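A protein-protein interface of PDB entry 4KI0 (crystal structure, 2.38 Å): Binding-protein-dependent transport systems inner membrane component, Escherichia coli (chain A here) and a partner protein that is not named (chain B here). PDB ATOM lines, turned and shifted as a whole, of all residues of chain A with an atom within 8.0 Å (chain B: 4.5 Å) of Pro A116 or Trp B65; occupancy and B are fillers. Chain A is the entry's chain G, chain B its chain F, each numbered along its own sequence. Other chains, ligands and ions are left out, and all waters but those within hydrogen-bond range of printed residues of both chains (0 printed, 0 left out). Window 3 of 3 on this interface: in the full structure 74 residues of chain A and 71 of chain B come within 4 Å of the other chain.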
ATOM      1  N   CYS A 106      23.003 -18.553  29.563  1.00  0.00           N
ATOM      2  CA  CYS A 106      23.919 -17.652  28.873  1.00  0.00           C
ATOM      3  C   CYS A 106      25.323 -18.256  28.736  1.00  0.00           C
ATOM      4  O   CYS A 106      25.891 -18.300  27.639  1.00  0.00           O
ATOM      5  CB  CYS A 106      24.014 -16.342  29.651  1.00  0.00           C
ATOM      6  SG  CYS A 106      23.913 -14.877  28.629  1.00  0.00           S
ATOM      7  N   ALA A 109      25.802 -21.095  26.097  1.00  0.00           N
ATOM      8  CA  ALA A 109      25.928 -20.592  24.731  1.00  0.00           C
ATOM      9  C   ALA A 109      27.323 -20.053  24.473  1.00  0.00           C
ATOM     10  O   ALA A 109      27.978 -20.439  23.506  1.00  0.00           O
ATOM     11  CB  ALA A 109      24.904 -19.504  24.471  1.00  0.00           C
ATOM     12  N   PHE A 110      27.778 -19.157  25.344  1.00  0.00           N
ATOM     13  CA  PHE A 110      29.103 -18.575  25.196  1.00  0.00           C
ATOM     14  C   PHE A 110      30.173 -19.667  25.169  1.00  0.00           C
ATOM     15  O   PHE A 110      31.078 -19.625  24.337  1.00  0.00           O
ATOM     16  CB  PHE A 110      29.396 -17.572  26.317  1.00  0.00           C
ATOM     17  CG  PHE A 110      28.661 -16.266  26.176  1.00  0.00           C
ATOM     18  CD1 PHE A 110      27.800 -15.823  27.164  1.00  0.00           C
ATOM     19  CD2 PHE A 110      28.832 -15.482  25.052  1.00  0.00           C
ATOM     20  CE1 PHE A 110      27.126 -14.618  27.026  1.00  0.00           C
ATOM     21  CE2 PHE A 110      28.165 -14.280  24.911  1.00  0.00           C
ATOM     22  CZ  PHE A 110      27.311 -13.845  25.895  1.00  0.00           C
ATOM     23  N   MET A 113      28.784 -22.698  21.953  1.00  0.00           N
ATOM     24  CA  MET A 113      28.143 -22.389  20.677  1.00  0.00           C
ATOM     25  C   MET A 113      28.835 -21.266  19.926  1.00  0.00           C
ATOM     26  O   MET A 113      29.465 -20.392  20.522  1.00  0.00           O
ATOM     27  CB  MET A 113      26.676 -22.031  20.897  1.00  0.00           C
ATOM     28  CG  MET A 113      25.914 -23.074  21.693  1.00  0.00           C
ATOM     29  SD  MET A 113      24.150 -22.740  21.765  1.00  0.00           S
ATOM     30  CE  MET A 113      23.646 -23.903  23.027  1.00  0.00           C
ATOM     31  N   ARG A 114      28.709 -21.317  18.605  1.00  0.00           N
ATOM     32  CA  ARG A 114      29.225 -20.287  17.720  1.00  0.00           C
ATOM     33  C   ARG A 114      28.107 -19.318  17.389  1.00  0.00           C
ATOM     34  O   ARG A 114      27.003 -19.736  17.042  1.00  0.00           O
ATOM     35  CB  ARG A 114      29.735 -20.901  16.412  1.00  0.00           C
ATOM     36  CG  ARG A 114      31.178 -21.380  16.441  1.00  0.00           C
ATOM     37  CD  ARG A 114      31.702 -21.609  15.027  1.00  0.00           C
ATOM     38  NE  ARG A 114      33.145 -21.385  14.937  1.00  0.00           N
ATOM     39  CZ  ARG A 114      33.819 -21.171  13.806  1.00  0.00           C
ATOM     40  NH1 ARG A 114      33.198 -21.146  12.627  1.00  0.00           N
ATOM     41  NH2 ARG A 114      35.133 -20.976  13.852  1.00  0.00           N
ATOM     42  N   PHE A 115      28.398 -18.028  17.498  1.00  0.00           N
ATOM     43  CA  PHE A 115      27.517 -16.989  16.971  1.00  0.00           C
ATOM     44  C   PHE A 115      28.296 -15.676  16.837  1.00  0.00           C
ATOM     45  O   PHE A 115      29.306 -15.484  17.515  1.00  0.00           O
ATOM     46  CB  PHE A 115      26.239 -16.837  17.823  1.00  0.00           C
ATOM     47  CG  PHE A 115      26.484 -16.680  19.298  1.00  0.00           C
ATOM     48  CD1 PHE A 115      26.531 -15.420  19.876  1.00  0.00           C
ATOM     49  CD2 PHE A 115      26.635 -17.792  20.112  1.00  0.00           C
ATOM     50  CE1 PHE A 115      26.745 -15.270  21.232  1.00  0.00           C
ATOM     51  CE2 PHE A 115      26.854 -17.651  21.468  1.00  0.00           C
ATOM     52  CZ  PHE A 115      26.909 -16.389  22.030  1.00  0.00           C
ATOM     53  N   PRO A 116      27.846 -14.778  15.942  1.00  0.00           N
ATOM     54  CA  PRO A 116      28.645 -13.585  15.652  1.00  0.00           C
ATOM     55  C   PRO A 116      28.601 -12.556  16.775  1.00  0.00           C
ATOM     56  O   PRO A 116      27.563 -12.386  17.418  1.00  0.00           O
ATOM     57  CB  PRO A 116      27.991 -13.029  14.382  1.00  0.00           C
ATOM     58  CG  PRO A 116      26.570 -13.466  14.470  1.00  0.00           C
ATOM     59  CD  PRO A 116      26.576 -14.789  15.189  1.00  0.00           C
ATOM     60  N   GLY A 117      29.723 -11.876  17.000  1.00  0.00           N
ATOM     61  CA  GLY A 117      29.818 -10.856  18.043  1.00  0.00           C
ATOM     62  C   GLY A 117      29.782 -11.452  19.438  1.00  0.00           C
ATOM     63  O   GLY A 117      29.363 -10.792  20.390  1.00  0.00           O
ATOM     64  N   LYS A 118      30.223 -12.703  19.550  1.00  0.00           N
ATOM     65  CA  LYS A 118      30.265 -13.413  20.823  1.00  0.00           C
ATOM     66  C   LYS A 118      31.380 -12.874  21.709  1.00  0.00           C
ATOM     67  O   LYS A 118      31.167 -12.612  22.896  1.00  0.00           O
ATOM     68  CB  LYS A 118      30.490 -14.900  20.580  1.00  0.00           C
ATOM     69  CG  LYS A 118      30.406 -15.738  21.837  1.00  0.00           C
ATOM     70  CD  LYS A 118      30.455 -17.221  21.525  1.00  0.00           C
ATOM     71  CE  LYS A 118      31.872 -17.749  21.507  1.00  0.00           C
ATOM     72  NZ  LYS A 118      31.845 -19.223  21.321  1.00  0.00           N
ATOM     73  N   ALA A 119      32.567 -12.728  21.124  1.00  0.00           N
ATOM     74  CA  ALA A 119      33.719 -12.140  21.810  1.00  0.00           C
ATOM     75  C   ALA A 119      33.450 -10.687  22.166  1.00  0.00           C
ATOM     76  O   ALA A 119      33.810 -10.230  23.253  1.00  0.00           O
ATOM     77  CB  ALA A 119      34.965 -12.241  20.944  1.00  0.00           C
ATOM     78  N   THR A 120      32.811  -9.968  21.248  1.00  0.00           N
ATOM     79  CA  THR A 120      32.400  -8.593  21.503  1.00  0.00           C
ATOM     80  C   THR A 120      31.384  -8.505  22.645  1.00  0.00           C
ATOM     81  O   THR A 120      31.529  -7.676  23.539  1.00  0.00           O
ATOM     82  CB  THR A 120      31.798  -7.951  20.239  1.00  0.00           C
ATOM     83  OG1 THR A 120      32.685  -8.163  19.135  1.00  0.00           O
ATOM     84  CG2 THR A 120      31.568  -6.452  20.442  1.00  0.00           C
ATOM     85  N   LEU A 121      30.363  -9.358  22.613  1.00  0.00           N
ATOM     86  CA  LEU A 121      29.334  -9.359  23.657  1.00  0.00           C
ATOM     87  C   LEU A 121      29.910  -9.597  25.045  1.00  0.00           C
ATOM     88  O   LEU A 121      29.540  -8.909  25.990  1.00  0.00           O
ATOM     89  CB  LEU A 121      28.255 -10.405  23.368  1.00  0.00           C
ATOM     90  CG  LEU A 121      27.118  -9.908  22.476  1.00  0.00           C
ATOM     91  CD1 LEU A 121      26.346 -11.074  21.879  1.00  0.00           C
ATOM     92  CD2 LEU A 121      26.193  -8.985  23.259  1.00  0.00           C
ATOM     93  N   ILE B  56      13.568 -14.945  17.701  1.00  0.00           N
ATOM     94  CA  ILE B  56      14.556 -15.932  18.127  1.00  0.00           C
ATOM     95  C   ILE B  56      13.935 -17.307  18.407  1.00  0.00           C
ATOM     96  O   ILE B  56      14.482 -18.327  17.997  1.00  0.00           O
ATOM     97  CB  ILE B  56      15.355 -15.411  19.342  1.00  0.00           C
ATOM     98  CG1 ILE B  56      16.411 -14.403  18.873  1.00  0.00           C
ATOM     99  CG2 ILE B  56      16.027 -16.549  20.090  1.00  0.00           C
ATOM    100  CD1 ILE B  56      16.944 -13.503  19.967  1.00  0.00           C
ATOM    101  N   ALA B  62      18.227 -19.472  14.874  1.00  0.00           N
ATOM    102  CA  ALA B  62      18.632 -18.564  15.941  1.00  0.00           C
ATOM    103  C   ALA B  62      18.724 -19.295  17.284  1.00  0.00           C
ATOM    104  O   ALA B  62      18.794 -18.650  18.330  1.00  0.00           O
ATOM    105  CB  ALA B  62      17.653 -17.406  16.034  1.00  0.00           C
ATOM    106  N   TYR B  63      18.738 -20.631  17.243  1.00  0.00           N
ATOM    107  CA  TYR B  63      18.774 -21.487  18.444  1.00  0.00           C
ATOM    108  C   TYR B  63      19.679 -20.942  19.534  1.00  0.00           C
ATOM    109  O   TYR B  63      19.244 -20.776  20.674  1.00  0.00           O
ATOM    110  CB  TYR B  63      19.229 -22.907  18.081  1.00  0.00           C
ATOM    111  CG  TYR B  63      19.095 -23.933  19.191  1.00  0.00           C
ATOM    112  CD1 TYR B  63      20.183 -24.281  19.981  1.00  0.00           C
ATOM    113  CD2 TYR B  63      17.886 -24.576  19.427  1.00  0.00           C
ATOM    114  CE1 TYR B  63      20.068 -25.230  20.984  1.00  0.00           C
ATOM    115  CE2 TYR B  63      17.760 -25.526  20.429  1.00  0.00           C
ATOM    116  CZ  TYR B  63      18.852 -25.850  21.207  1.00  0.00           C
ATOM    117  OH  TYR B  63      18.724 -26.793  22.203  1.00  0.00           O
ATOM    118  N   ALA B  64      20.928 -20.648  19.180  1.00  0.00           N
ATOM    119  CA  ALA B  64      21.918 -20.196  20.164  1.00  0.00           C
ATOM    120  C   ALA B  64      21.457 -18.980  20.945  1.00  0.00           C
ATOM    121  O   ALA B  64      21.664 -18.903  22.151  1.00  0.00           O
ATOM    122  CB  ALA B  64      23.246 -19.904  19.491  1.00  0.00           C
ATOM    123  N   TRP B  65      20.823 -18.039  20.258  1.00  0.00           N
ATOM    124  CA  TRP B  65      20.390 -16.782  20.867  1.00  0.00           C
ATOM    125  C   TRP B  65      19.266 -16.962  21.889  1.00  0.00           C
ATOM    126  O   TRP B  65      19.023 -16.067  22.696  1.00  0.00           O
ATOM    127  CB  TRP B  65      19.962 -15.781  19.779  1.00  0.00           C
ATOM    128  CG  TRP B  65      21.096 -15.383  18.888  1.00  0.00           C
ATOM    129  CD1 TRP B  65      21.467 -15.977  17.711  1.00  0.00           C
ATOM    130  CD2 TRP B  65      22.032 -14.325  19.116  1.00  0.00           C
ATOM    131  NE1 TRP B  65      22.571 -15.346  17.189  1.00  0.00           N
ATOM    132  CE2 TRP B  65      22.937 -14.327  18.032  1.00  0.00           C
ATOM    133  CE3 TRP B  65      22.188 -13.369  20.126  1.00  0.00           C
ATOM    134  CZ2 TRP B  65      23.989 -13.409  17.932  1.00  0.00           C
ATOM    135  CZ3 TRP B  65      23.234 -12.459  20.029  1.00  0.00           C
ATOM    136  CH2 TRP B  65      24.121 -12.487  18.938  1.00  0.00           C
ATOM    137  N   ARG B  66      18.585 -18.107  21.850  1.00  0.00           N
ATOM    138  CA  ARG B  66      17.547 -18.436  22.830  1.00  0.00           C
ATOM    139  C   ARG B  66      18.120 -18.536  24.236  1.00  0.00           C
ATOM    140  O   ARG B  66      17.454 -18.187  25.209  1.00  0.00           O
ATOM    141  CB  ARG B  66      16.872 -19.757  22.476  1.00  0.00           C
ATOM    142  CG  ARG B  66      16.091 -19.704  21.183  1.00  0.00           C
ATOM    143  CD  ARG B  66      15.562 -21.064  20.778  1.00  0.00           C
ATOM    144  NE  ARG B  66      14.960 -21.010  19.449  1.00  0.00           N
ATOM    145  CZ  ARG B  66      14.440 -22.056  18.815  1.00  0.00           C
ATOM    146  NH1 ARG B  66      14.441 -23.256  19.384  1.00  0.00           N
ATOM    147  NH2 ARG B  66      13.915 -21.899  17.609  1.00  0.00           N
ATOM    148  N   TYR B  67      19.361 -19.005  24.328  1.00  0.00           N
ATOM    149  CA  TYR B  67      20.066 -19.138  25.600  1.00  0.00           C
ATOM    150  C   TYR B  67      20.593 -17.807  26.110  1.00  0.00           C
ATOM    151  O   TYR B  67      20.771 -17.617  27.323  1.00  0.00           O
ATOM    152  CB  TYR B  67      21.240 -20.108  25.439  1.00  0.00           C
ATOM    153  CG  TYR B  67      20.830 -21.551  25.286  1.00  0.00           C
ATOM    154  CD1 TYR B  67      20.377 -22.030  24.074  1.00  0.00           C
ATOM    155  CD2 TYR B  67      20.905 -22.438  26.359  1.00  0.00           C
ATOM    156  CE1 TYR B  67      19.998 -23.349  23.922  1.00  0.00           C
ATOM    157  CE2 TYR B  67      20.526 -23.762  26.215  1.00  0.00           C
ATOM    158  CZ  TYR B  67      20.075 -24.210  24.993  1.00  0.00           C
ATOM    159  OH  TYR B  67      19.697 -25.516  24.815  1.00  0.00           O
ATOM    160  N   VAL B  68      20.862 -16.891  25.186  1.00  0.00           N
ATOM    161  CA  VAL B  68      21.546 -15.635  25.514  1.00  0.00           C
ATOM    162  C   VAL B  68      20.563 -14.482  25.736  1.00  0.00           C
ATOM    163  O   VAL B  68      20.814 -13.596  26.542  1.00  0.00           O
ATOM    164  CB  VAL B  68      22.566 -15.278  24.407  1.00  0.00           C
ATOM    165  CG1 VAL B  68      23.272 -13.962  24.701  1.00  0.00           C
ATOM    166  CG2 VAL B  68      23.592 -16.388  24.270  1.00  0.00           C
ATOM    167  N   TYR B  69      19.438 -14.516  25.036  1.00  0.00           N
ATOM    168  CA  TYR B  69      18.501 -13.386  25.001  1.00  0.00           C
ATOM    169  C   TYR B  69      17.898 -13.014  26.360  1.00  0.00           C
ATOM    170  O   TYR B  69      17.883 -11.837  26.711  1.00  0.00           O
ATOM    171  CB  TYR B  69      17.402 -13.661  23.964  1.00  0.00           C
ATOM    172  CG  TYR B  69      16.222 -12.726  24.005  1.00  0.00           C
ATOM    173  CD1 TYR B  69      15.056 -13.084  24.673  1.00  0.00           C
ATOM    174  CD2 TYR B  69      16.257 -11.496  23.353  1.00  0.00           C
ATOM    175  CE1 TYR B  69      13.960 -12.243  24.701  1.00  0.00           C
ATOM    176  CE2 TYR B  69      15.168 -10.645  23.379  1.00  0.00           C
ATOM    177  CZ  TYR B  69      14.021 -11.026  24.055  1.00  0.00           C
ATOM    178  OH  TYR B  69      12.931 -10.194  24.090  1.00  0.00           O
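The side-chain hydroxyl of Tyr B63 lies within hydrogen-bond range of the side-chain hydroxyl of Tyr B67. O of Met A113 lies within hydrogen-bond range of NZ of Lys A118 (2.8 Å).
Printed residues of chain B within 4 Å of Cys A106: Tyr B67 and Val B68. Printed residues of chain B within 4 Å of Ala A109: Tyr B67 (3.8 Å) and Val B68 (3.4 Å). Of chain B, only Trp B65 (3.8 Å) comes within 4 Å of Pro A116. Trp B65 touches just these residues of chain A: Phe A115, Pro A116 and Leu A121. Arg B66 touches none of the printed residues of chain A. Of the printed residues of chain A, Tyr B67 touches Cys A106 (3.3 Å), Ala A109 (3.8 Å) and Met A113 (3.8 Å). The nearest residue of chain A that does not touch Trp B65 is Gly A117 (5.7 Å). The nearest printed residue of chain B that does not touch Cys A106 is Tyr B69 (5.8 Å).
O of Tyr B67 sits at hydrogen-bond distance from N of Cys A106, 3.3 Å away.
Printed residues of chain A that touch a printed residue of chain B: Cys A106, Ala A109, Met A113, Phe A115, Pro A116 and Leu A121. Of the 9 printed residues of chain B, 4 touch a printed residue of chain A. Hydrophobic or aromatic side chains of chain B within 4 Å of the printed part of chain A: Ala B64, Trp B65, Tyr B67 and Val B68. Among the printed residues, 9 pairs touch across the chains. Among the printed residues, no Asp or Glu carboxylate lies within 4 Å of a Lys or Arg side-chain nitrogen of the other chain.
SG of Cys A106 touches O of Val B68 (3.9 Å). CB of Ala A109 touches CB of Tyr B67, at 3.8 Å. Ala A109 touches Val B68. Met A113 touches Ala B64. CE1 of Tyr B67 touches CE of Met A113 (3.8 Å). Trp B65 touches Phe A115. Pro A116 touches Trp B65 (O to CZ2, 3.8 Å). CD1 of Leu A121 touches CZ3 of Trp B65 (3.9 Å).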
